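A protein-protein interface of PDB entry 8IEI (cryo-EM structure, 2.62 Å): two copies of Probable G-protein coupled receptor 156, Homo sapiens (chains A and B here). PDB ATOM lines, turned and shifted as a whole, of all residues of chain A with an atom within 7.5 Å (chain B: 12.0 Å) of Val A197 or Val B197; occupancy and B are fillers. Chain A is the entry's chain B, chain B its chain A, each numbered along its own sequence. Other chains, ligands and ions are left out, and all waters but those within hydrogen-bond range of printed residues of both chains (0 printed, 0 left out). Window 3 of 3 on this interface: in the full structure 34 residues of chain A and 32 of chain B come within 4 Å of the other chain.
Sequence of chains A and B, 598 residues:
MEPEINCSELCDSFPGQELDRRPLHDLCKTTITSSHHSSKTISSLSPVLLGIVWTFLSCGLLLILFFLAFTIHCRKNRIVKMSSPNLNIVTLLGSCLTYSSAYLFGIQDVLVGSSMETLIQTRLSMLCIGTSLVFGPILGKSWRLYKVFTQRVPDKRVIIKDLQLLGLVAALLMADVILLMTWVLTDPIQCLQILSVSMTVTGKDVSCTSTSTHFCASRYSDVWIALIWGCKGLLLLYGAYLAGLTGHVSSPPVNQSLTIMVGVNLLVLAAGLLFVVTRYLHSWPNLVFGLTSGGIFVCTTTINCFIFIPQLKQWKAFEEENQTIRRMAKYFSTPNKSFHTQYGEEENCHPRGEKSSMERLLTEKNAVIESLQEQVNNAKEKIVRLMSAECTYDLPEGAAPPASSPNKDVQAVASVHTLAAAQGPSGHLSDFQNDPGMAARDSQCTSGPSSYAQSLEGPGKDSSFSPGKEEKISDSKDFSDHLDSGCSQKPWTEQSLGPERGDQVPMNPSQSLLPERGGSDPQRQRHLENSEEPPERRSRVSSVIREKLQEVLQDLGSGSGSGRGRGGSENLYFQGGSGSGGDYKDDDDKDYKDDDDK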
ATOM      1  N   LEU A 195      25.712 -10.779  28.882  1.00  0.00           N
ATOM      2  CA  LEU A 195      24.292 -10.986  29.125  1.00  0.00           C
ATOM      3  C   LEU A 195      23.891 -12.244  28.371  1.00  0.00           C
ATOM      4  O   LEU A 195      24.245 -12.407  27.199  1.00  0.00           O
ATOM      5  CB  LEU A 195      23.465  -9.767  28.696  1.00  0.00           C
ATOM      6  CG  LEU A 195      23.422  -9.285  27.241  1.00  0.00           C
ATOM      7  CD1 LEU A 195      22.365 -10.007  26.402  1.00  0.00           C
ATOM      8  CD2 LEU A 195      23.192  -7.780  27.195  1.00  0.00           C
ATOM      9  N   SER A 196      23.211 -13.154  29.061  1.00  0.00           N
ATOM     10  CA  SER A 196      22.939 -14.469  28.503  1.00  0.00           C
ATOM     11  C   SER A 196      21.655 -15.019  29.097  1.00  0.00           C
ATOM     12  O   SER A 196      21.339 -14.764  30.262  1.00  0.00           O
ATOM     13  CB  SER A 196      24.097 -15.435  28.776  1.00  0.00           C
ATOM     14  OG  SER A 196      23.983 -16.014  30.064  1.00  0.00           O
ATOM     15  N   VAL A 197      20.921 -15.772  28.280  1.00  0.00           N
ATOM     16  CA  VAL A 197      19.732 -16.499  28.706  1.00  0.00           C
ATOM     17  C   VAL A 197      20.002 -17.981  28.496  1.00  0.00           C
ATOM     18  O   VAL A 197      20.358 -18.403  27.389  1.00  0.00           O
ATOM     19  CB  VAL A 197      18.474 -16.039  27.944  1.00  0.00           C
ATOM     20  CG1 VAL A 197      18.105 -14.621  28.350  1.00  0.00           C
ATOM     21  CG2 VAL A 197      18.659 -16.127  26.425  1.00  0.00           C
ATOM     22  N   SER A 198      19.854 -18.764  29.561  1.00  0.00           N
ATOM     23  CA  SER A 198      20.188 -20.181  29.560  1.00  0.00           C
ATOM     24  C   SER A 198      18.920 -20.998  29.740  1.00  0.00           C
ATOM     25  O   SER A 198      18.141 -20.746  30.666  1.00  0.00           O
ATOM     26  CB  SER A 198      21.194 -20.508  30.667  1.00  0.00           C
ATOM     27  OG  SER A 198      22.422 -19.836  30.450  1.00  0.00           O
ATOM     28  N   MET A 199      18.722 -21.974  28.858  1.00  0.00           N
ATOM     29  CA  MET A 199      17.556 -22.853  28.868  1.00  0.00           C
ATOM     30  C   MET A 199      18.061 -24.265  29.140  1.00  0.00           C
ATOM     31  O   MET A 199      18.316 -25.037  28.213  1.00  0.00           O
ATOM     32  CB  MET A 199      16.801 -22.763  27.542  1.00  0.00           C
ATOM     33  CG  MET A 199      16.122 -21.420  27.314  1.00  0.00           C
ATOM     34  SD  MET A 199      15.283 -21.309  25.722  1.00  0.00           S
ATOM     35  CE  MET A 199      16.635 -20.809  24.659  1.00  0.00           C
ATOM     36  N   THR A 200      18.205 -24.598  30.419  1.00  0.00           N
ATOM     37  CA  THR A 200      18.689 -25.903  30.832  1.00  0.00           C
ATOM     38  C   THR A 200      17.523 -26.867  31.021  1.00  0.00           C
ATOM     39  O   THR A 200      16.367 -26.464  31.170  1.00  0.00           O
ATOM     40  CB  THR A 200      19.497 -25.796  32.129  1.00  0.00           C
ATOM     41  OG1 THR A 200      20.257 -26.995  32.323  1.00  0.00           O
ATOM     42  CG2 THR A 200      18.581 -25.576  33.330  1.00  0.00           C
ATOM     43  N   CYS A 208      14.530 -22.095  33.003  1.00  0.00           N
ATOM     44  CA  CYS A 208      15.182 -21.049  32.226  1.00  0.00           C
ATOM     45  C   CYS A 208      15.700 -19.971  33.166  1.00  0.00           C
ATOM     46  O   CYS A 208      15.029 -19.607  34.135  1.00  0.00           O
ATOM     47  CB  CYS A 208      14.219 -20.432  31.207  1.00  0.00           C
ATOM     48  SG  CYS A 208      13.453 -21.625  30.087  1.00  0.00           S
ATOM     49  N   THR A 209      16.896 -19.465  32.870  1.00  0.00           N
ATOM     50  CA  THR A 209      17.539 -18.434  33.670  1.00  0.00           C
ATOM     51  C   THR A 209      18.077 -17.343  32.757  1.00  0.00           C
ATOM     52  O   THR A 209      18.399 -17.586  31.591  1.00  0.00           O
ATOM     53  CB  THR A 209      18.687 -19.005  34.517  1.00  0.00           C
ATOM     54  OG1 THR A 209      19.565 -19.773  33.685  1.00  0.00           O
ATOM     55  CG2 THR A 209      18.144 -19.888  35.628  1.00  0.00           C
ATOM     56  N   SER A 210      18.169 -16.131  33.305  1.00  0.00           N
ATOM     57  CA  SER A 210      18.679 -14.967  32.578  1.00  0.00           C
ATOM     58  C   SER A 210      19.588 -14.204  33.535  1.00  0.00           C
ATOM     59  O   SER A 210      19.104 -13.508  34.432  1.00  0.00           O
ATOM     60  CB  SER A 210      17.542 -14.089  32.071  1.00  0.00           C
ATOM     61  OG  SER A 210      16.578 -14.857  31.373  1.00  0.00           O
ATOM     62  N   THR A 211      20.898 -14.338  33.338  1.00  0.00           N
ATOM     63  CA  THR A 211      21.899 -13.751  34.218  1.00  0.00           C
ATOM     64  C   THR A 211      22.829 -12.851  33.420  1.00  0.00           C
ATOM     65  O   THR A 211      23.166 -13.149  32.271  1.00  0.00           O
ATOM     66  CB  THR A 211      22.720 -14.836  34.924  1.00  0.00           C
ATOM     67  OG1 THR A 211      23.336 -15.685  33.947  1.00  0.00           O
ATOM     68  CG2 THR A 211      21.835 -15.671  35.836  1.00  0.00           C
ATOM     69  N   SER A 212      23.232 -11.743  34.040  1.00  0.00           N
ATOM     70  CA  SER A 212      24.232 -10.838  33.491  1.00  0.00           C
ATOM     71  C   SER A 212      25.287 -10.591  34.557  1.00  0.00           C
ATOM     72  O   SER A 212      24.951 -10.252  35.696  1.00  0.00           O
ATOM     73  CB  SER A 212      23.605  -9.516  33.040  1.00  0.00           C
ATOM     74  OG  SER A 212      24.461  -8.820  32.152  1.00  0.00           O
ATOM     75  N   GLN B 193      21.775 -30.628  30.192  1.00  0.00           N
ATOM     76  CA  GLN B 193      21.877 -30.164  28.813  1.00  0.00           C
ATOM     77  C   GLN B 193      21.723 -28.648  28.821  1.00  0.00           C
ATOM     78  O   GLN B 193      20.627 -28.131  29.065  1.00  0.00           O
ATOM     79  CB  GLN B 193      20.814 -30.817  27.933  1.00  0.00           C
ATOM     80  CG  GLN B 193      21.044 -32.292  27.669  1.00  0.00           C
ATOM     81  CD  GLN B 193      19.969 -32.897  26.792  1.00  0.00           C
ATOM     82  OE1 GLN B 193      19.013 -32.222  26.410  1.00  0.00           O
ATOM     83  NE2 GLN B 193      20.120 -34.175  26.466  1.00  0.00           N
ATOM     84  N   ILE B 194      22.816 -27.942  28.554  1.00  0.00           N
ATOM     85  CA  ILE B 194      22.852 -26.485  28.598  1.00  0.00           C
ATOM     86  C   ILE B 194      22.900 -25.979  27.164  1.00  0.00           C
ATOM     87  O   ILE B 194      23.899 -26.169  26.462  1.00  0.00           O
ATOM     88  CB  ILE B 194      24.051 -25.973  29.410  1.00  0.00           C
ATOM     89  CG1 ILE B 194      23.877 -26.308  30.896  1.00  0.00           C
ATOM     90  CG2 ILE B 194      24.243 -24.470  29.206  1.00  0.00           C
ATOM     91  CD1 ILE B 194      22.954 -25.366  31.645  1.00  0.00           C
ATOM     92  N   LEU B 195      21.819 -25.338  26.730  1.00  0.00           N
ATOM     93  CA  LEU B 195      21.776 -24.598  25.477  1.00  0.00           C
ATOM     94  C   LEU B 195      21.426 -23.157  25.808  1.00  0.00           C
ATOM     95  O   LEU B 195      20.494 -22.903  26.579  1.00  0.00           O
ATOM     96  CB  LEU B 195      20.773 -25.219  24.495  1.00  0.00           C
ATOM     97  CG  LEU B 195      19.282 -25.283  24.850  1.00  0.00           C
ATOM     98  CD1 LEU B 195      18.517 -24.044  24.390  1.00  0.00           C
ATOM     99  CD2 LEU B 195      18.659 -26.542  24.262  1.00  0.00           C
ATOM    100  N   SER B 196      22.194 -22.220  25.261  1.00  0.00           N
ATOM    101  CA  SER B 196      22.064 -20.826  25.656  1.00  0.00           C
ATOM    102  C   SER B 196      22.637 -19.937  24.565  1.00  0.00           C
ATOM    103  O   SER B 196      23.389 -20.389  23.697  1.00  0.00           O
ATOM    104  CB  SER B 196      22.774 -20.559  26.986  1.00  0.00           C
ATOM    105  OG  SER B 196      24.180 -20.646  26.838  1.00  0.00           O
ATOM    106  N   VAL B 197      22.262 -18.662  24.625  1.00  0.00           N
ATOM    107  CA  VAL B 197      22.799 -17.624  23.756  1.00  0.00           C
ATOM    108  C   VAL B 197      23.284 -16.484  24.638  1.00  0.00           C
ATOM    109  O   VAL B 197      22.556 -16.018  25.522  1.00  0.00           O
ATOM    110  CB  VAL B 197      21.755 -17.128  22.731  1.00  0.00           C
ATOM    111  CG1 VAL B 197      21.404 -18.242  21.758  1.00  0.00           C
ATOM    112  CG2 VAL B 197      20.498 -16.598  23.423  1.00  0.00           C
ATOM    113  N   SER B 198      24.522 -16.048  24.407  1.00  0.00           N
ATOM    114  CA  SER B 198      25.157 -15.025  25.222  1.00  0.00           C
ATOM    115  C   SER B 198      25.756 -13.956  24.324  1.00  0.00           C
ATOM    116  O   SER B 198      26.338 -14.265  23.279  1.00  0.00           O
ATOM    117  CB  SER B 198      26.252 -15.623  26.114  1.00  0.00           C
ATOM    118  OG  SER B 198      27.401 -15.953  25.354  1.00  0.00           O
ATOM    119  N   MET B 199      25.607 -12.700  24.738  1.00  0.00           N
ATOM    120  CA  MET B 199      26.202 -11.555  24.062  1.00  0.00           C
ATOM    121  C   MET B 199      27.360 -11.065  24.920  1.00  0.00           C
ATOM    122  O   MET B 199      27.159 -10.699  26.083  1.00  0.00           O
ATOM    123  CB  MET B 199      25.160 -10.453  23.847  1.00  0.00           C
ATOM    124  CG  MET B 199      25.695  -9.099  23.365  1.00  0.00           C
ATOM    125  SD  MET B 199      24.433  -7.815  23.427  1.00  0.00           S
ATOM    126  CE  MET B 199      23.748  -7.936  21.776  1.00  0.00           C
ATOM    127  N   THR B 200      28.560 -11.054  24.347  1.00  0.00           N
ATOM    128  CA  THR B 200      29.765 -10.636  25.051  1.00  0.00           C
ATOM    129  C   THR B 200      30.012  -9.161  24.766  1.00  0.00           C
ATOM    130  O   THR B 200      30.046  -8.749  23.601  1.00  0.00           O
ATOM    131  CB  THR B 200      30.971 -11.470  24.623  1.00  0.00           C
ATOM    132  OG1 THR B 200      31.322 -11.148  23.272  1.00  0.00           O
ATOM    133  CG2 THR B 200      30.663 -12.958  24.718  1.00  0.00           C
ATOM    134  N   VAL B 201      30.179  -8.372  25.824  1.00  0.00           N
ATOM    135  CA  VAL B 201      30.455  -6.943  25.720  1.00  0.00           C
ATOM    136  C   VAL B 201      31.747  -6.688  26.485  1.00  0.00           C
ATOM    137  O   VAL B 201      31.758  -6.679  27.722  1.00  0.00           O
ATOM    138  CB  VAL B 201      29.307  -6.085  26.262  1.00  0.00           C
ATOM    139  CG1 VAL B 201      29.536  -4.617  25.923  1.00  0.00           C
ATOM    140  CG2 VAL B 201      27.972  -6.563  25.703  1.00  0.00           C
ATOM    141  N   VAL B 206      31.130  -6.360  20.207  1.00  0.00           N
ATOM    142  CA  VAL B 206      29.979  -7.169  20.594  1.00  0.00           C
ATOM    143  C   VAL B 206      30.013  -8.450  19.774  1.00  0.00           C
ATOM    144  O   VAL B 206      30.136  -8.402  18.543  1.00  0.00           O
ATOM    145  CB  VAL B 206      28.655  -6.416  20.386  1.00  0.00           C
ATOM    146  CG1 VAL B 206      27.467  -7.359  20.536  1.00  0.00           C
ATOM    147  CG2 VAL B 206      28.548  -5.256  21.365  1.00  0.00           C
ATOM    148  N   SER B 207      29.910  -9.591  20.453  1.00  0.00           N
ATOM    149  CA  SER B 207      29.885 -10.898  19.812  1.00  0.00           C
ATOM    150  C   SER B 207      28.792 -11.749  20.439  1.00  0.00           C
ATOM    151  O   SER B 207      28.623 -11.757  21.662  1.00  0.00           O
ATOM    152  CB  SER B 207      31.237 -11.610  19.941  1.00  0.00           C
ATOM    153  OG  SER B 207      31.283 -12.765  19.122  1.00  0.00           O
ATOM    154  N   CYS B 208      28.053 -12.464  19.592  1.00  0.00           N
ATOM    155  CA  CYS B 208      26.981 -13.355  20.015  1.00  0.00           C
ATOM    156  C   CYS B 208      27.355 -14.783  19.652  1.00  0.00           C
ATOM    157  O   CYS B 208      27.800 -15.045  18.530  1.00  0.00           O
ATOM    158  CB  CYS B 208      25.653 -12.972  19.360  1.00  0.00           C
ATOM    159  SG  CYS B 208      25.019 -11.354  19.857  1.00  0.00           S
ATOM    160  N   THR B 209      27.177 -15.700  20.603  1.00  0.00           N
ATOM    161  CA  THR B 209      27.494 -17.108  20.413  1.00  0.00           C
ATOM    162  C   THR B 209      26.337 -17.960  20.912  1.00  0.00           C
ATOM    163  O   THR B 209      25.668 -17.604  21.887  1.00  0.00           O
ATOM    164  CB  THR B 209      28.783 -17.494  21.152  1.00  0.00           C
ATOM    165  OG1 THR B 209      29.771 -16.474  20.957  1.00  0.00           O
ATOM    166  CG2 THR B 209      29.323 -18.822  20.638  1.00  0.00           C
ATOM    167  N   SER B 210      26.102 -19.079  20.231  1.00  0.00           N
ATOM    168  CA  SER B 210      25.080 -20.053  20.604  1.00  0.00           C
ATOM    169  C   SER B 210      25.770 -21.395  20.809  1.00  0.00           C
ATOM    170  O   SER B 210      26.308 -21.971  19.859  1.00  0.00           O
ATOM    171  CB  SER B 210      23.996 -20.148  19.533  1.00  0.00           C
ATOM    172  OG  SER B 210      23.502 -18.865  19.191  1.00  0.00           O
ATOM    173  N   THR B 211      25.752 -21.887  22.046  1.00  0.00           N
ATOM    174  CA  THR B 211      26.436 -23.117  22.424  1.00  0.00           C
ATOM    175  C   THR B 211      25.447 -24.069  23.080  1.00  0.00           C
ATOM    176  O   THR B 211      24.674 -23.661  23.952  1.00  0.00           O
ATOM    177  CB  THR B 211      27.597 -22.831  23.380  1.00  0.00           C
ATOM    178  OG1 THR B 211      27.126 -22.059  24.492  1.00  0.00           O
ATOM    179  CG2 THR B 211      28.702 -22.068  22.667  1.00  0.00           C
ATOM    180  N   SER B 212      25.478 -25.330  22.655  1.00  0.00           N
ATOM    181  CA  SER B 212      24.692 -26.405  23.255  1.00  0.00           C
ATOM    182  C   SER B 212      25.680 -27.383  23.880  1.00  0.00           C
ATOM    183  O   SER B 212      26.246 -28.234  23.189  1.00  0.00           O
ATOM    184  CB  SER B 212      23.805 -27.084  22.215  1.00  0.00           C
ATOM    185  OG  SER B 212      22.808 -27.878  22.834  1.00  0.00           O
ATOM    186  N   THR B 213      25.881 -27.257  25.190  1.00  0.00           N
ATOM    187  CA  THR B 213      26.887 -28.017  25.919  1.00  0.00           C
ATOM    188  C   THR B 213      26.220 -28.997  26.873  1.00  0.00           C
ATOM    189  O   THR B 213      25.201 -28.680  27.494  1.00  0.00           O
ATOM    190  CB  THR B 213      27.812 -27.087  26.709  1.00  0.00           C
ATOM    191  OG1 THR B 213      27.053 -26.380  27.698  1.00  0.00           O
ATOM    192  CG2 THR B 213      28.493 -26.091  25.781  1.00  0.00           C
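The side-chain hydroxyl (OG1) of Thr A200 sits close to the backbone carbonyl oxygen (O) of Gln B193 (3.5 Å).
The backbone NH (N) of Met A199 lies within hydrogen-bond range of the backbone carbonyl oxygen (O) of Leu B195, at 3.0 Å.
O of Val B197 sits at hydrogen-bond distance from N of Val A197 (3.2 Å).
The backbone NH (N) of Met B199 lies within hydrogen-bond range of the backbone carbonyl oxygen (O) of Leu A195.
The backbone carbonyl oxygen (O) of Ile B194 is in hydrogen-bond range of the backbone NH (N) of Thr B213 (2.6 Å).
N of Ser B196 lies within hydrogen-bond range of O of Thr B211 (3.2 Å).
The backbone carbonyl oxygen (O) of Ser B198 is in hydrogen-bond range of the backbone NH (N) of Thr B209 (3.2 Å).
N of Thr A211 lies within hydrogen-bond range of O of Ser A196 (3.1 Å).
O of Thr A209 lies within hydrogen-bond range of N of Ser A198 (2.8 Å).
CA of Ser B198 touches O of Leu A195, at 3.4 Å.
Val B197 touches Ser A196.
CB of Ser A196 touches CB of Ser B198 (3.4 Å).
Val A197 touches Ser B196.
OG of Ser A198 touches CB of Ser B196, 3.6 Å away.
Gln B193 touches Met A199 (O to O, 3.95 Å).
Thr A200 touches Ile B194 (OG1 to CD1, 3.2 Å).
Of chain B, only Val B197 and Ser B198 come within 4 Å of Ser A196.
Of chain B, only Ser B196 and Val B197 come within 4 Å of Val A197.
Of the printed residues of chain B, Ser A198 touches Ser B196.
Met A199 touches just these residues of chain B: Gln B193 (3.95 Å) and Leu B195 (3.0 Å).
No residue of chain B comes within 4 Å of Thr A209.
No residue of chain B comes within 4 Å of Ser A210.
Of the printed residues of chain A, Leu B195 touches Met A199 (3.0 Å).
Of chain A, only Ser A196 and Val A197 come within 4 Å of Val B197.
Thr B211 touches none of the printed residues of chain A.
The nearest residue of chain B that does not touch Val A197 is Leu B195 (4.6 Å).
Of the 11 printed residues of chain A, 6 touch a printed residue of chain B.
Printed residues of chain A that touch a printed residue of chain B: Leu A195, Ser A196, Val A197, Ser A198, Met A199 and Thr A200.
Of the 17 printed residues of chain B, 7 touch a printed residue of chain A.
Among the printed residues, 11 pairs touch across the chains.
Leu A195 touches Ser B198, but with the chains exchanged Ser A198 does not touch Leu B195 (4.01 Å).
Leu A195 touches Met B199, and with the chains exchanged Met A199 touches Leu B195.
Ser A196 touches Ser B198, and with the chains exchanged Ser A198 touches Ser B196.
Val A197 touches its own counterpart, Val B197.
Positions printed for both chains: 195, 196, 197, 198, 199, 200, 208, 209, 210, 211 and 212.
Of the 11 pairs that touch across the chains among the printed residues, 7 have their exchanged pair printed and touching as well.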
